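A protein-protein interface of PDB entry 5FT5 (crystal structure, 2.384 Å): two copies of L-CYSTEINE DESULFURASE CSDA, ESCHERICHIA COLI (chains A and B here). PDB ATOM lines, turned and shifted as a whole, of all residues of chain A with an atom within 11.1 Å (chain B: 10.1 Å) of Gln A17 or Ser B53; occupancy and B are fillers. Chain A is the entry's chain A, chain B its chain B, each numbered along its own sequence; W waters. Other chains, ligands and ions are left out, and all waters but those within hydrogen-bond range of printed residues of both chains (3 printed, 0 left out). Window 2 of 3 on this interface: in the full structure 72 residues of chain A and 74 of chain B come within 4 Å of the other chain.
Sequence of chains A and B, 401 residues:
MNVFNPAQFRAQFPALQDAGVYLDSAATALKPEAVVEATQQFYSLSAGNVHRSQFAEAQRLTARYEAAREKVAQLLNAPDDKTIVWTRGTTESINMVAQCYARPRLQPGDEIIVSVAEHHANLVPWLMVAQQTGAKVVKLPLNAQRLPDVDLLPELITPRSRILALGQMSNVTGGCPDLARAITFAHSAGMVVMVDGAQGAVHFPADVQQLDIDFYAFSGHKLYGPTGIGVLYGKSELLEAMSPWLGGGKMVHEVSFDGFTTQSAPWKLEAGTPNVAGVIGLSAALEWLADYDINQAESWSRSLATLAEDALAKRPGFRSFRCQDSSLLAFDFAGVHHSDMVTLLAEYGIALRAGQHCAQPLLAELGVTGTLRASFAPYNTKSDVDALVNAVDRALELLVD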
ATOM      1  N   ARG A  10      20.331   4.953  27.143  1.00  0.00           N
ATOM      2  CA  ARG A  10      20.471   5.284  25.729  1.00  0.00           C
ATOM      3  C   ARG A  10      19.249   4.888  24.903  1.00  0.00           C
ATOM      4  O   ARG A  10      19.058   5.383  23.792  1.00  0.00           O
ATOM      5  CB  ARG A  10      21.759   4.696  25.140  1.00  0.00           C
ATOM      6  CG  ARG A  10      21.804   3.197  25.121  1.00  0.00           C
ATOM      7  CD  ARG A  10      23.019   2.704  24.372  1.00  0.00           C
ATOM      8  NE  ARG A  10      23.078   1.248  24.401  1.00  0.00           N
ATOM      9  CZ  ARG A  10      23.680   0.544  25.352  1.00  0.00           C
ATOM     10  NH1 ARG A  10      24.291   1.164  26.356  1.00  0.00           N
ATOM     11  NH2 ARG A  10      23.673  -0.782  25.299  1.00  0.00           N
ATOM     12  N   ALA A  11      18.407   4.021  25.456  1.00  0.00           N
ATOM     13  CA  ALA A  11      17.184   3.615  24.763  1.00  0.00           C
ATOM     14  C   ALA A  11      16.184   4.764  24.621  1.00  0.00           C
ATOM     15  O   ALA A  11      15.175   4.635  23.925  1.00  0.00           O
ATOM     16  CB  ALA A  11      16.536   2.431  25.470  1.00  0.00           C
ATOM     17  N   GLN A  12      16.470   5.887  25.274  1.00  0.00           N
ATOM     18  CA  GLN A  12      15.542   7.015  25.302  1.00  0.00           C
ATOM     19  C   GLN A  12      15.804   8.013  24.182  1.00  0.00           C
ATOM     20  O   GLN A  12      15.066   8.984  24.023  1.00  0.00           O
ATOM     21  CB  GLN A  12      15.630   7.736  26.650  1.00  0.00           C
ATOM     22  CG  GLN A  12      15.284   6.867  27.839  1.00  0.00           C
ATOM     23  CD  GLN A  12      13.811   6.539  27.902  1.00  0.00           C
ATOM     24  OE1 GLN A  12      13.426   5.391  28.118  1.00  0.00           O
ATOM     25  NE2 GLN A  12      12.973   7.553  27.710  1.00  0.00           N
ATOM     26  N   PHE A  13      16.862   7.777  23.414  1.00  0.00           N
ATOM     27  CA  PHE A  13      17.290   8.727  22.392  1.00  0.00           C
ATOM     28  C   PHE A  13      16.946   8.262  20.980  1.00  0.00           C
ATOM     29  O   PHE A  13      17.646   7.430  20.405  1.00  0.00           O
ATOM     30  CB  PHE A  13      18.789   9.008  22.532  1.00  0.00           C
ATOM     31  CG  PHE A  13      19.145   9.736  23.795  1.00  0.00           C
ATOM     32  CD1 PHE A  13      19.215   9.060  25.003  1.00  0.00           C
ATOM     33  CD2 PHE A  13      19.383  11.102  23.783  1.00  0.00           C
ATOM     34  CE1 PHE A  13      19.531   9.728  26.175  1.00  0.00           C
ATOM     35  CE2 PHE A  13      19.701  11.778  24.952  1.00  0.00           C
ATOM     36  CZ  PHE A  13      19.772  11.088  26.148  1.00  0.00           C
ATOM     37  N   PRO A  14      15.862   8.813  20.413  1.00  0.00           N
ATOM     38  CA  PRO A  14      15.366   8.413  19.091  1.00  0.00           C
ATOM     39  C   PRO A  14      16.396   8.600  17.978  1.00  0.00           C
ATOM     40  O   PRO A  14      16.239   8.013  16.909  1.00  0.00           O
ATOM     41  CB  PRO A  14      14.166   9.344  18.871  1.00  0.00           C
ATOM     42  CG  PRO A  14      14.388  10.493  19.804  1.00  0.00           C
ATOM     43  CD  PRO A  14      15.056   9.898  20.996  1.00  0.00           C
ATOM     44  N   ALA A  15      17.432   9.394  18.225  1.00  0.00           N
ATOM     45  CA  ALA A  15      18.436   9.677  17.202  1.00  0.00           C
ATOM     46  C   ALA A  15      19.579   8.665  17.179  1.00  0.00           C
ATOM     47  O   ALA A  15      20.394   8.667  16.256  1.00  0.00           O
ATOM     48  CB  ALA A  15      18.989  11.086  17.371  1.00  0.00           C
ATOM     49  N   LEU A  16      19.640   7.797  18.183  1.00  0.00           N
ATOM     50  CA  LEU A  16      20.797   6.918  18.333  1.00  0.00           C
ATOM     51  C   LEU A  16      21.161   6.109  17.085  1.00  0.00           C
ATOM     52  O   LEU A  16      22.312   6.133  16.652  1.00  0.00           O
ATOM     53  CB  LEU A  16      20.653   6.001  19.553  1.00  0.00           C
ATOM     54  CG  LEU A  16      21.351   6.491  20.828  1.00  0.00           C
ATOM     55  CD1 LEU A  16      21.662   5.316  21.742  1.00  0.00           C
ATOM     56  CD2 LEU A  16      22.615   7.281  20.507  1.00  0.00           C
ATOM     57  N   GLN A  17      20.199   5.396  16.508  1.00  0.00           N
ATOM     58  CA  GLN A  17      20.503   4.558  15.350  1.00  0.00           C
ATOM     59  C   GLN A  17      21.159   5.346  14.217  1.00  0.00           C
ATOM     60  O   GLN A  17      22.253   5.005  13.763  1.00  0.00           O
ATOM     61  CB  GLN A  17      19.256   3.842  14.830  1.00  0.00           C
ATOM     62  CG  GLN A  17      19.553   2.933  13.644  1.00  0.00           C
ATOM     63  CD  GLN A  17      18.366   2.087  13.223  1.00  0.00           C
ATOM     64  OE1 GLN A  17      17.238   2.307  13.666  1.00  0.00           O
ATOM     65  NE2 GLN A  17      18.617   1.107  12.359  1.00  0.00           N
ATOM     66  N   ASP A  18      20.488   6.401  13.767  1.00  0.00           N
ATOM     67  CA  ASP A  18      20.981   7.214  12.662  1.00  0.00           C
ATOM     68  C   ASP A  18      22.338   7.851  12.958  1.00  0.00           C
ATOM     69  O   ASP A  18      23.175   7.986  12.066  1.00  0.00           O
ATOM     70  CB  ASP A  18      19.964   8.302  12.306  1.00  0.00           C
ATOM     71  CG  ASP A  18      20.523   9.338  11.346  1.00  0.00           C
ATOM     72  OD1 ASP A  18      20.681   9.018  10.147  1.00  0.00           O
ATOM     73  OD2 ASP A  18      20.799  10.474  11.787  1.00  0.00           O
ATOM     74  N   ALA A  19      22.545   8.228  14.215  1.00  0.00           N
ATOM     75  CA  ALA A  19      23.717   9.006  14.616  1.00  0.00           C
ATOM     76  C   ALA A  19      25.031   8.219  14.621  1.00  0.00           C
ATOM     77  O   ALA A  19      26.107   8.800  14.751  1.00  0.00           O
ATOM     78  CB  ALA A  19      23.477   9.646  15.985  1.00  0.00           C
ATOM     79  N   GLY A  20      24.942   6.900  14.486  1.00  0.00           N
ATOM     80  CA  GLY A  20      26.122   6.058  14.542  1.00  0.00           C
ATOM     81  C   GLY A  20      26.849   6.182  15.870  1.00  0.00           C
ATOM     82  O   GLY A  20      26.243   6.065  16.934  1.00  0.00           O
ATOM     83  N   VAL A  21      28.154   6.417  15.807  1.00  0.00           N
ATOM     84  CA  VAL A  21      28.955   6.602  17.009  1.00  0.00           C
ATOM     85  C   VAL A  21      29.101   8.093  17.298  1.00  0.00           C
ATOM     86  O   VAL A  21      30.005   8.753  16.781  1.00  0.00           O
ATOM     87  CB  VAL A  21      30.336   5.948  16.860  1.00  0.00           C
ATOM     88  CG1 VAL A  21      31.175   6.155  18.121  1.00  0.00           C
ATOM     89  CG2 VAL A  21      30.174   4.470  16.555  1.00  0.00           C
ATOM     90  N   TYR A  22      28.195   8.617  18.119  1.00  0.00           N
ATOM     91  CA  TYR A  22      28.102  10.052  18.343  1.00  0.00           C
ATOM     92  C   TYR A  22      29.047  10.532  19.445  1.00  0.00           C
ATOM     93  O   TYR A  22      28.835  10.259  20.629  1.00  0.00           O
ATOM     94  CB  TYR A  22      26.656  10.446  18.658  1.00  0.00           C
ATOM     95  CG  TYR A  22      26.447  11.938  18.725  1.00  0.00           C
ATOM     96  CD1 TYR A  22      26.291  12.693  17.567  1.00  0.00           C
ATOM     97  CD2 TYR A  22      26.412  12.597  19.947  1.00  0.00           C
ATOM     98  CE1 TYR A  22      26.100  14.064  17.626  1.00  0.00           C
ATOM     99  CE2 TYR A  22      26.225  13.963  20.017  1.00  0.00           C
ATOM    100  CZ  TYR A  22      26.071  14.691  18.855  1.00  0.00           C
ATOM    101  OH  TYR A  22      25.887  16.053  18.929  1.00  0.00           O
ATOM    102  N   LEU A  30      22.361  14.980  22.156  1.00  0.00           N
ATOM    103  CA  LEU A  30      21.160  14.328  21.648  1.00  0.00           C
ATOM    104  C   LEU A  30      20.017  14.509  22.640  1.00  0.00           C
ATOM    105  O   LEU A  30      20.256  14.719  23.831  1.00  0.00           O
ATOM    106  CB  LEU A  30      21.425  12.839  21.434  1.00  0.00           C
ATOM    107  CG  LEU A  30      22.534  12.556  20.425  1.00  0.00           C
ATOM    108  CD1 LEU A  30      22.719  11.062  20.234  1.00  0.00           C
ATOM    109  CD2 LEU A  30      22.222  13.254  19.103  1.00  0.00           C
ATOM    110  N   LYS A  31      18.779  14.418  22.159  1.00  0.00           N
ATOM    111  CA  LYS A  31      17.625  14.650  23.025  1.00  0.00           C
ATOM    112  C   LYS A  31      16.869  13.361  23.345  1.00  0.00           C
ATOM    113  O   LYS A  31      16.674  12.516  22.477  1.00  0.00           O
ATOM    114  CB  LYS A  31      16.671  15.675  22.400  1.00  0.00           C
ATOM    115  CG  LYS A  31      17.342  16.748  21.528  1.00  0.00           C
ATOM    116  CD  LYS A  31      18.352  17.583  22.302  1.00  0.00           C
ATOM    117  CE  LYS A  31      18.994  18.641  21.409  1.00  0.00           C
ATOM    118  NZ  LYS A  31      20.048  19.416  22.126  1.00  0.00           N
ATOM    119  N   ALA A 346      34.045  10.234   9.787  1.00  0.00           N
ATOM    120  CA  ALA A 346      32.618  10.328   9.528  1.00  0.00           C
ATOM    121  C   ALA A 346      32.158   9.210   8.585  1.00  0.00           C
ATOM    122  O   ALA A 346      31.068   8.666   8.744  1.00  0.00           O
ATOM    123  CB  ALA A 346      32.263  11.697   8.963  1.00  0.00           C
ATOM    124  N   TYR A 348      33.374   6.371   8.526  1.00  0.00           N
ATOM    125  CA  TYR A 348      33.389   5.176   9.355  1.00  0.00           C
ATOM    126  C   TYR A 348      32.301   5.250  10.414  1.00  0.00           C
ATOM    127  O   TYR A 348      32.210   4.394  11.286  1.00  0.00           O
ATOM    128  CB  TYR A 348      34.770   4.955   9.983  1.00  0.00           C
ATOM    129  CG  TYR A 348      35.656   4.087   9.123  1.00  0.00           C
ATOM    130  CD1 TYR A 348      36.294   4.604   8.003  1.00  0.00           C
ATOM    131  CD2 TYR A 348      35.820   2.739   9.406  1.00  0.00           C
ATOM    132  CE1 TYR A 348      37.086   3.802   7.198  1.00  0.00           C
ATOM    133  CE2 TYR A 348      36.609   1.931   8.608  1.00  0.00           C
ATOM    134  CZ  TYR A 348      37.238   2.468   7.508  1.00  0.00           C
ATOM    135  OH  TYR A 348      38.022   1.667   6.717  1.00  0.00           O
ATOM    136  N   GLY A 349      31.470   6.280  10.330  1.00  0.00           N
ATOM    137  CA  GLY A 349      30.324   6.399  11.209  1.00  0.00           C
ATOM    138  C   GLY A 349      30.632   6.982  12.573  1.00  0.00           C
ATOM    139  O   GLY A 349      29.825   6.871  13.497  1.00  0.00           O
ATOM    140  N   ILE A 350      31.799   7.604  12.704  1.00  0.00           N
ATOM    141  CA  ILE A 350      32.174   8.263  13.952  1.00  0.00           C
ATOM    142  C   ILE A 350      31.922   9.758  13.836  1.00  0.00           C
ATOM    143  O   ILE A 350      32.481  10.417  12.961  1.00  0.00           O
ATOM    144  CB  ILE A 350      33.665   8.060  14.280  1.00  0.00           C
ATOM    145  CG1 ILE A 350      34.095   6.624  13.977  1.00  0.00           C
ATOM    146  CG2 ILE A 350      33.945   8.432  15.730  1.00  0.00           C
ATOM    147  CD1 ILE A 350      33.399   5.594  14.821  1.00  0.00           C
ATOM    148  N   ALA A 351      31.091  10.293  14.723  1.00  0.00           N
ATOM    149  CA  ALA A 351      30.766  11.715  14.686  1.00  0.00           C
ATOM    150  C   ALA A 351      31.550  12.525  15.723  1.00  0.00           C
ATOM    151  O   ALA A 351      31.291  12.434  16.925  1.00  0.00           O
ATOM    152  CB  ALA A 351      29.260  11.929  14.864  1.00  0.00           C
ATOM    153  N   TYR A 379      25.206   7.891  26.916  1.00  0.00           N
ATOM    154  CA  TYR A 379      24.581   7.044  25.894  1.00  0.00           C
ATOM    155  C   TYR A 379      25.579   6.381  24.936  1.00  0.00           C
ATOM    156  O   TYR A 379      25.178   5.678  24.009  1.00  0.00           O
ATOM    157  CB  TYR A 379      23.460   7.769  25.126  1.00  0.00           C
ATOM    158  CG  TYR A 379      23.790   9.165  24.639  1.00  0.00           C
ATOM    159  CD1 TYR A 379      24.930   9.414  23.891  1.00  0.00           C
ATOM    160  CD2 TYR A 379      22.935  10.229  24.904  1.00  0.00           C
ATOM    161  CE1 TYR A 379      25.220  10.686  23.438  1.00  0.00           C
ATOM    162  CE2 TYR A 379      23.217  11.501  24.456  1.00  0.00           C
ATOM    163  CZ  TYR A 379      24.360  11.724  23.725  1.00  0.00           C
ATOM    164  OH  TYR A 379      24.642  12.997  23.286  1.00  0.00           O
ATOM    165  N   ASN A 380      26.870   6.606  25.169  1.00  0.00           N
ATOM    166  CA  ASN A 380      27.920   5.880  24.454  1.00  0.00           C
ATOM    167  C   ASN A 380      28.199   4.516  25.093  1.00  0.00           C
ATOM    168  O   ASN A 380      27.819   4.272  26.237  1.00  0.00           O
ATOM    169  CB  ASN A 380      29.214   6.697  24.412  1.00  0.00           C
ATOM    170  CG  ASN A 380      29.080   7.970  23.602  1.00  0.00           C
ATOM    171  OD1 ASN A 380      29.269   9.072  24.120  1.00  0.00           O
ATOM    172  ND2 ASN A 380      28.764   7.825  22.319  1.00  0.00           N
ATOM    173  N   THR A 381      28.881   3.641  24.357  1.00  0.00           N
ATOM    174  CA  THR A 381      29.153   2.283  24.817  1.00  0.00           C
ATOM    175  C   THR A 381      30.629   1.912  24.648  1.00  0.00           C
ATOM    176  O   THR A 381      31.403   2.671  24.066  1.00  0.00           O
ATOM    177  CB  THR A 381      28.314   1.254  24.026  1.00  0.00           C
ATOM    178  OG1 THR A 381      28.800   1.174  22.678  1.00  0.00           O
ATOM    179  CG2 THR A 381      26.841   1.645  24.014  1.00  0.00           C
ATOM    180  N   ASP A 384      31.338   1.674  21.099  1.00  0.00           N
ATOM    181  CA  ASP A 384      31.678   2.964  20.507  1.00  0.00           C
ATOM    182  C   ASP A 384      33.192   3.189  20.500  1.00  0.00           C
ATOM    183  O   ASP A 384      33.763   3.590  19.482  1.00  0.00           O
ATOM    184  CB  ASP A 384      30.980   4.105  21.249  1.00  0.00           C
ATOM    185  CG  ASP A 384      29.480   4.136  21.003  1.00  0.00           C
ATOM    186  OD1 ASP A 384      29.000   3.448  20.073  1.00  0.00           O
ATOM    187  OD2 ASP A 384      28.779   4.867  21.734  1.00  0.00           O
ATOM    188  N   SER B  44      14.884  14.779  16.546  1.00  0.00           N
ATOM    189  CA  SER B  44      14.966  13.321  16.439  1.00  0.00           C
ATOM    190  C   SER B  44      16.169  12.901  15.608  1.00  0.00           C
ATOM    191  O   SER B  44      16.380  11.717  15.354  1.00  0.00           O
ATOM    192  CB  SER B  44      13.698  12.751  15.800  1.00  0.00           C
ATOM    193  OG  SER B  44      12.563  12.953  16.619  1.00  0.00           O
ATOM    194  N   LEU B  45      16.951  13.883  15.178  1.00  0.00           N
ATOM    195  CA  LEU B  45      18.037  13.635  14.248  1.00  0.00           C
ATOM    196  C   LEU B  45      19.328  14.229  14.784  1.00  0.00           C
ATOM    197  O   LEU B  45      19.329  15.314  15.364  1.00  0.00           O
ATOM    198  CB  LEU B  45      17.699  14.254  12.892  1.00  0.00           C
ATOM    199  CG  LEU B  45      17.898  13.391  11.650  1.00  0.00           C
ATOM    200  CD1 LEU B  45      17.420  11.979  11.918  1.00  0.00           C
ATOM    201  CD2 LEU B  45      17.139  13.995  10.479  1.00  0.00           C
ATOM    202  N   SER B  46      20.429  13.514  14.598  1.00  0.00           N
ATOM    203  CA  SER B  46      21.723  14.005  15.046  1.00  0.00           C
ATOM    204  C   SER B  46      22.091  15.242  14.241  1.00  0.00           C
ATOM    205  O   SER B  46      21.785  15.326  13.051  1.00  0.00           O
ATOM    206  CB  SER B  46      22.789  12.920  14.883  1.00  0.00           C
ATOM    207  OG  SER B  46      24.064  13.393  15.273  1.00  0.00           O
ATOM    208  N   VAL B  50      27.285  12.583  10.792  1.00  0.00           N
ATOM    209  CA  VAL B  50      27.018  11.185  10.466  1.00  0.00           C
ATOM    210  C   VAL B  50      25.526  10.850  10.441  1.00  0.00           C
ATOM    211  O   VAL B  50      24.758  11.296  11.295  1.00  0.00           O
ATOM    212  CB  VAL B  50      27.761  10.219  11.418  1.00  0.00           C
ATOM    213  CG1 VAL B  50      27.338   8.778  11.151  1.00  0.00           C
ATOM    214  CG2 VAL B  50      29.270  10.380  11.264  1.00  0.00           C
ATOM    215  N   HIS B  51      25.126  10.062   9.450  1.00  0.00           N
ATOM    216  CA  HIS B  51      23.745   9.615   9.336  1.00  0.00           C
ATOM    217  C   HIS B  51      23.687   8.238   8.695  1.00  0.00           C
ATOM    218  O   HIS B  51      23.813   8.097   7.474  1.00  0.00           O
ATOM    219  CB  HIS B  51      22.912  10.624   8.542  1.00  0.00           C
ATOM    220  CG  HIS B  51      22.953  12.008   9.106  1.00  0.00           C
ATOM    221  ND1 HIS B  51      22.261  12.370  10.243  1.00  0.00           N
ATOM    222  CD2 HIS B  51      23.617  13.116   8.702  1.00  0.00           C
ATOM    223  CE1 HIS B  51      22.487  13.645  10.507  1.00  0.00           C
ATOM    224  NE2 HIS B  51      23.307  14.121   9.587  1.00  0.00           N
ATOM    225  N   ARG B  52      23.476   7.228   9.533  1.00  0.00           N
ATOM    226  CA  ARG B  52      23.531   5.830   9.117  1.00  0.00           C
ATOM    227  C   ARG B  52      22.230   5.316   8.486  1.00  0.00           C
ATOM    228  O   ARG B  52      22.242   4.343   7.726  1.00  0.00           O
ATOM    229  CB  ARG B  52      23.901   4.944  10.316  1.00  0.00           C
ATOM    230  CG  ARG B  52      25.207   5.312  11.024  1.00  0.00           C
ATOM    231  CD  ARG B  52      26.430   4.952  10.200  1.00  0.00           C
ATOM    232  NE  ARG B  52      26.290   3.642   9.567  1.00  0.00           N
ATOM    233  CZ  ARG B  52      26.429   2.477  10.195  1.00  0.00           C
ATOM    234  NH1 ARG B  52      26.711   2.440  11.492  1.00  0.00           N
ATOM    235  NH2 ARG B  52      26.279   1.341   9.522  1.00  0.00           N
ATOM    236  N   SER B  53      21.107   5.953   8.798  1.00  0.00           N
ATOM    237  CA  SER B  53      19.818   5.431   8.344  1.00  0.00           C
ATOM    238  C   SER B  53      18.801   6.498   7.952  1.00  0.00           C
ATOM    239  O   SER B  53      17.716   6.172   7.478  1.00  0.00           O
ATOM    240  CB  SER B  53      19.215   4.505   9.408  1.00  0.00           C
ATOM    241  OG  SER B  53      19.136   5.149  10.668  1.00  0.00           O
ATOM    242  N   GLN B  54      19.149   7.766   8.148  1.00  0.00           N
ATOM    243  CA  GLN B  54      18.236   8.862   7.831  1.00  0.00           C
ATOM    244  C   GLN B  54      18.954  10.027   7.166  1.00  0.00           C
ATOM    245  O   GLN B  54      18.669  11.185   7.445  1.00  0.00           O
ATOM    246  CB  GLN B  54      17.513   9.335   9.092  1.00  0.00           C
ATOM    247  CG  GLN B  54      16.701   8.240   9.760  1.00  0.00           C
ATOM    248  CD  GLN B  54      15.903   8.747  10.939  1.00  0.00           C
ATOM    249  OE1 GLN B  54      16.065   8.271  12.060  1.00  0.00           O
ATOM    250  NE2 GLN B  54      15.030   9.718  10.690  1.00  0.00           N
ATOM    251  N   PHE B  55      19.881   9.705   6.273  1.00  0.00           N
ATOM    252  CA  PHE B  55      20.675  10.712   5.581  1.00  0.00           C
ATOM    253  C   PHE B  55      19.792  11.686   4.802  1.00  0.00           C
ATOM    254  O   PHE B  55      19.970  12.904   4.884  1.00  0.00           O
ATOM    255  CB  PHE B  55      21.668  10.029   4.639  1.00  0.00           C
ATOM    256  CG  PHE B  55      22.960  10.771   4.480  1.00  0.00           C
ATOM    257  CD1 PHE B  55      23.049  12.114   4.800  1.00  0.00           C
ATOM    258  CD2 PHE B  55      24.089  10.124   4.008  1.00  0.00           C
ATOM    259  CE1 PHE B  55      24.235  12.796   4.654  1.00  0.00           C
ATOM    260  CE2 PHE B  55      25.280  10.804   3.858  1.00  0.00           C
ATOM    261  CZ  PHE B  55      25.353  12.142   4.182  1.00  0.00           C
ATOM    262  N   ALA B  56      18.841  11.143   4.047  1.00  0.00           N
ATOM    263  CA  ALA B  56      17.935  11.959   3.245  1.00  0.00           C
ATOM    264  C   ALA B  56      17.221  13.002   4.095  1.00  0.00           C
ATOM    265  O   ALA B  56      17.240  14.192   3.781  1.00  0.00           O
ATOM    266  CB  ALA B  56      16.922  11.078   2.512  1.00  0.00           C
ATOM    267  N   GLU B  57      16.586  12.556   5.172  1.00  0.00           N
ATOM    268  CA  GLU B  57      15.894  13.478   6.059  1.00  0.00           C
ATOM    269  C   GLU B  57      16.826  14.589   6.514  1.00  0.00           C
ATOM    270  O   GLU B  57      16.491  15.766   6.430  1.00  0.00           O
ATOM    271  CB  GLU B  57      15.342  12.748   7.281  1.00  0.00           C
ATOM    272  CG  GLU B  57      14.159  11.855   6.995  1.00  0.00           C
ATOM    273  CD  GLU B  57      13.446  11.431   8.265  1.00  0.00           C
ATOM    274  OE1 GLU B  57      13.575  12.152   9.282  1.00  0.00           O
ATOM    275  OE2 GLU B  57      12.762  10.382   8.243  1.00  0.00           O
ATOM    276  N   ALA B  58      17.998  14.206   6.999  1.00  0.00           N
ATOM    277  CA  ALA B  58      18.962  15.167   7.524  1.00  0.00           C
ATOM    278  C   ALA B  58      19.364  16.201   6.477  1.00  0.00           C
ATOM    279  O   ALA B  58      19.477  17.389   6.783  1.00  0.00           O
ATOM    280  CB  ALA B  58      20.190  14.447   8.066  1.00  0.00           C
ATOM    281  N   GLN B  59      19.586  15.749   5.247  1.00  0.00           N
ATOM    282  CA  GLN B  59      20.002  16.644   4.176  1.00  0.00           C
ATOM    283  C   GLN B  59      18.918  17.677   3.881  1.00  0.00           C
ATOM    284  O   GLN B  59      19.216  18.799   3.477  1.00  0.00           O
ATOM    285  CB  GLN B  59      20.357  15.859   2.909  1.00  0.00           C
ATOM    286  CG  GLN B  59      21.622  15.028   3.033  1.00  0.00           C
ATOM    287  CD  GLN B  59      22.025  14.362   1.727  1.00  0.00           C
ATOM    288  OE1 GLN B  59      23.143  14.546   1.247  1.00  0.00           O
ATOM    289  NE2 GLN B  59      21.120  13.576   1.155  1.00  0.00           N
HETATM  290  O   HOH W   1      28.428   3.871  13.097  1.00  0.00           O
HETATM  291  O   HOH W   2      29.176   4.544   8.442  1.00  0.00           O
HETATM  292  O   HOH W   3      26.035  11.811  13.866  1.00  0.00           O
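No position is printed for both chains.
Printed residues of chain B that touch a printed residue of chain A: Ser B44, Leu B45, Ser B46, Val B50, His B51, Arg B52, Ser B53 and Gln B54.
Hydrophobic or aromatic side chains of chain B within 4 Å of the printed part of chain A: Leu B45, Val B50 and His B51.
Along chain B the printed residues that touch a printed residue of chain A span positions 44 to 54.
Printed residues of chain A that touch a printed residue of chain B: Ala A15, Gln A17, Asp A18, Ala A19, Gly A20, Tyr A22, Ala A346, Gly A349, Ile A350 and Ala A351.
Among the printed residues, no Asp or Glu carboxylate lies within 4 Å of a Lys or Arg side-chain nitrogen of the other chain.
Among the printed residues, merely in contact across the chains: Tyr A22 with Ser B46 (3.2 Å), Ala A15 with Ser B44 (3.4 Å), Ala A19 with Ser B46 (3.5 Å), Ala A346 with Val B50 (3.5 Å), Ile A350 with Val B50 (3.6 Å), Asp A18 with Leu B45 (3.7 Å), Gly A20 with Arg B52 (3.7 Å), Gln A17 with Ser B53 (3.7 Å), Asp A18 with Val B50 (3.7 Å), Ala A19 with Val B50 (3.8 Å), Gly A349 with Val B50 (3.8 Å), Gln A17 with Arg B52 (3.8 Å), Ala A351 with Val B50 (3.9 Å) and Ala A15 with Ser B46 (3.96 Å).
Water W1 bridges the guanidinium group (NH1) of Arg B52 and the backbone carbonyl oxygen (O) of Gly A349.
Water W3 lies within hydrogen-bond range of the side-chain hydroxyl of Ser B46 (2.9 Å), the backbone carbonyl oxygen of Val B50 (2.9 Å) and the backbone carbonyl oxygen of Ala A19 (3.1 Å).
Water W2 lies within hydrogen-bond range of NE of Arg B52 (3.2 Å) and N of Gly A349 (3.4 Å).
N of Ser B53 is in hydrogen-bond range of OD1 of Asp A18.
OD2 of Asp A18 is in hydrogen-bond range of ND1 of His B51, at 2.8 Å.
The side-chain carboxylate (OD1) of Asp A18 sits at hydrogen-bond distance from the backbone NH (N) of Gln B54, at 2.8 Å.
O of Asp A18 lies within hydrogen-bond range of N of Arg B52, at 2.7 Å.
The side-chain carboxylate of Glu B57 is in hydrogen-bond range of the side-chain amide nitrogen of Gln B54.
The backbone carbonyl oxygen (O) of Tyr A22 sits at hydrogen-bond distance from the side-chain amide nitrogen (ND2) of Asn A380 (3.0 Å).
N of Ala A351 lies within hydrogen-bond range of O of Val A21 (2.8 Å).
N of Val A21 lies within hydrogen-bond range of O of Gly A349.
Gln A17 touches just these residues of chain B: Arg B52 (3.8 Å) and Ser B53 (3.7 Å).
Of chain B, only Ser B44 and Ser B46 come within 4 Å of Ala A15.
No residue of chain B comes within 4 Å of Leu A16.
Of chain B, only Ser B46 and Val B50 come within 4 Å of Ala A19.
Of chain A, only Asp A18 (2.8 Å) comes within 4 Å of Gln B54.
Of the printed residues of chain A, Leu B45 touches Asp A18.
Printed residues of chain B within 4 Å of Ala A346: Val B50.
Printed residues of chain A within 4 Å of His B51: Asp A18.
Printed residues of chain B within 4 Å of Ile A350: Val B50.
Ala B56 touches none of the printed residues of chain A.
Gln B59 touches none of the printed residues of chain A.
The nearest residue of chain B that does not touch Gln A17 is Gln B54 (6.1 Å).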
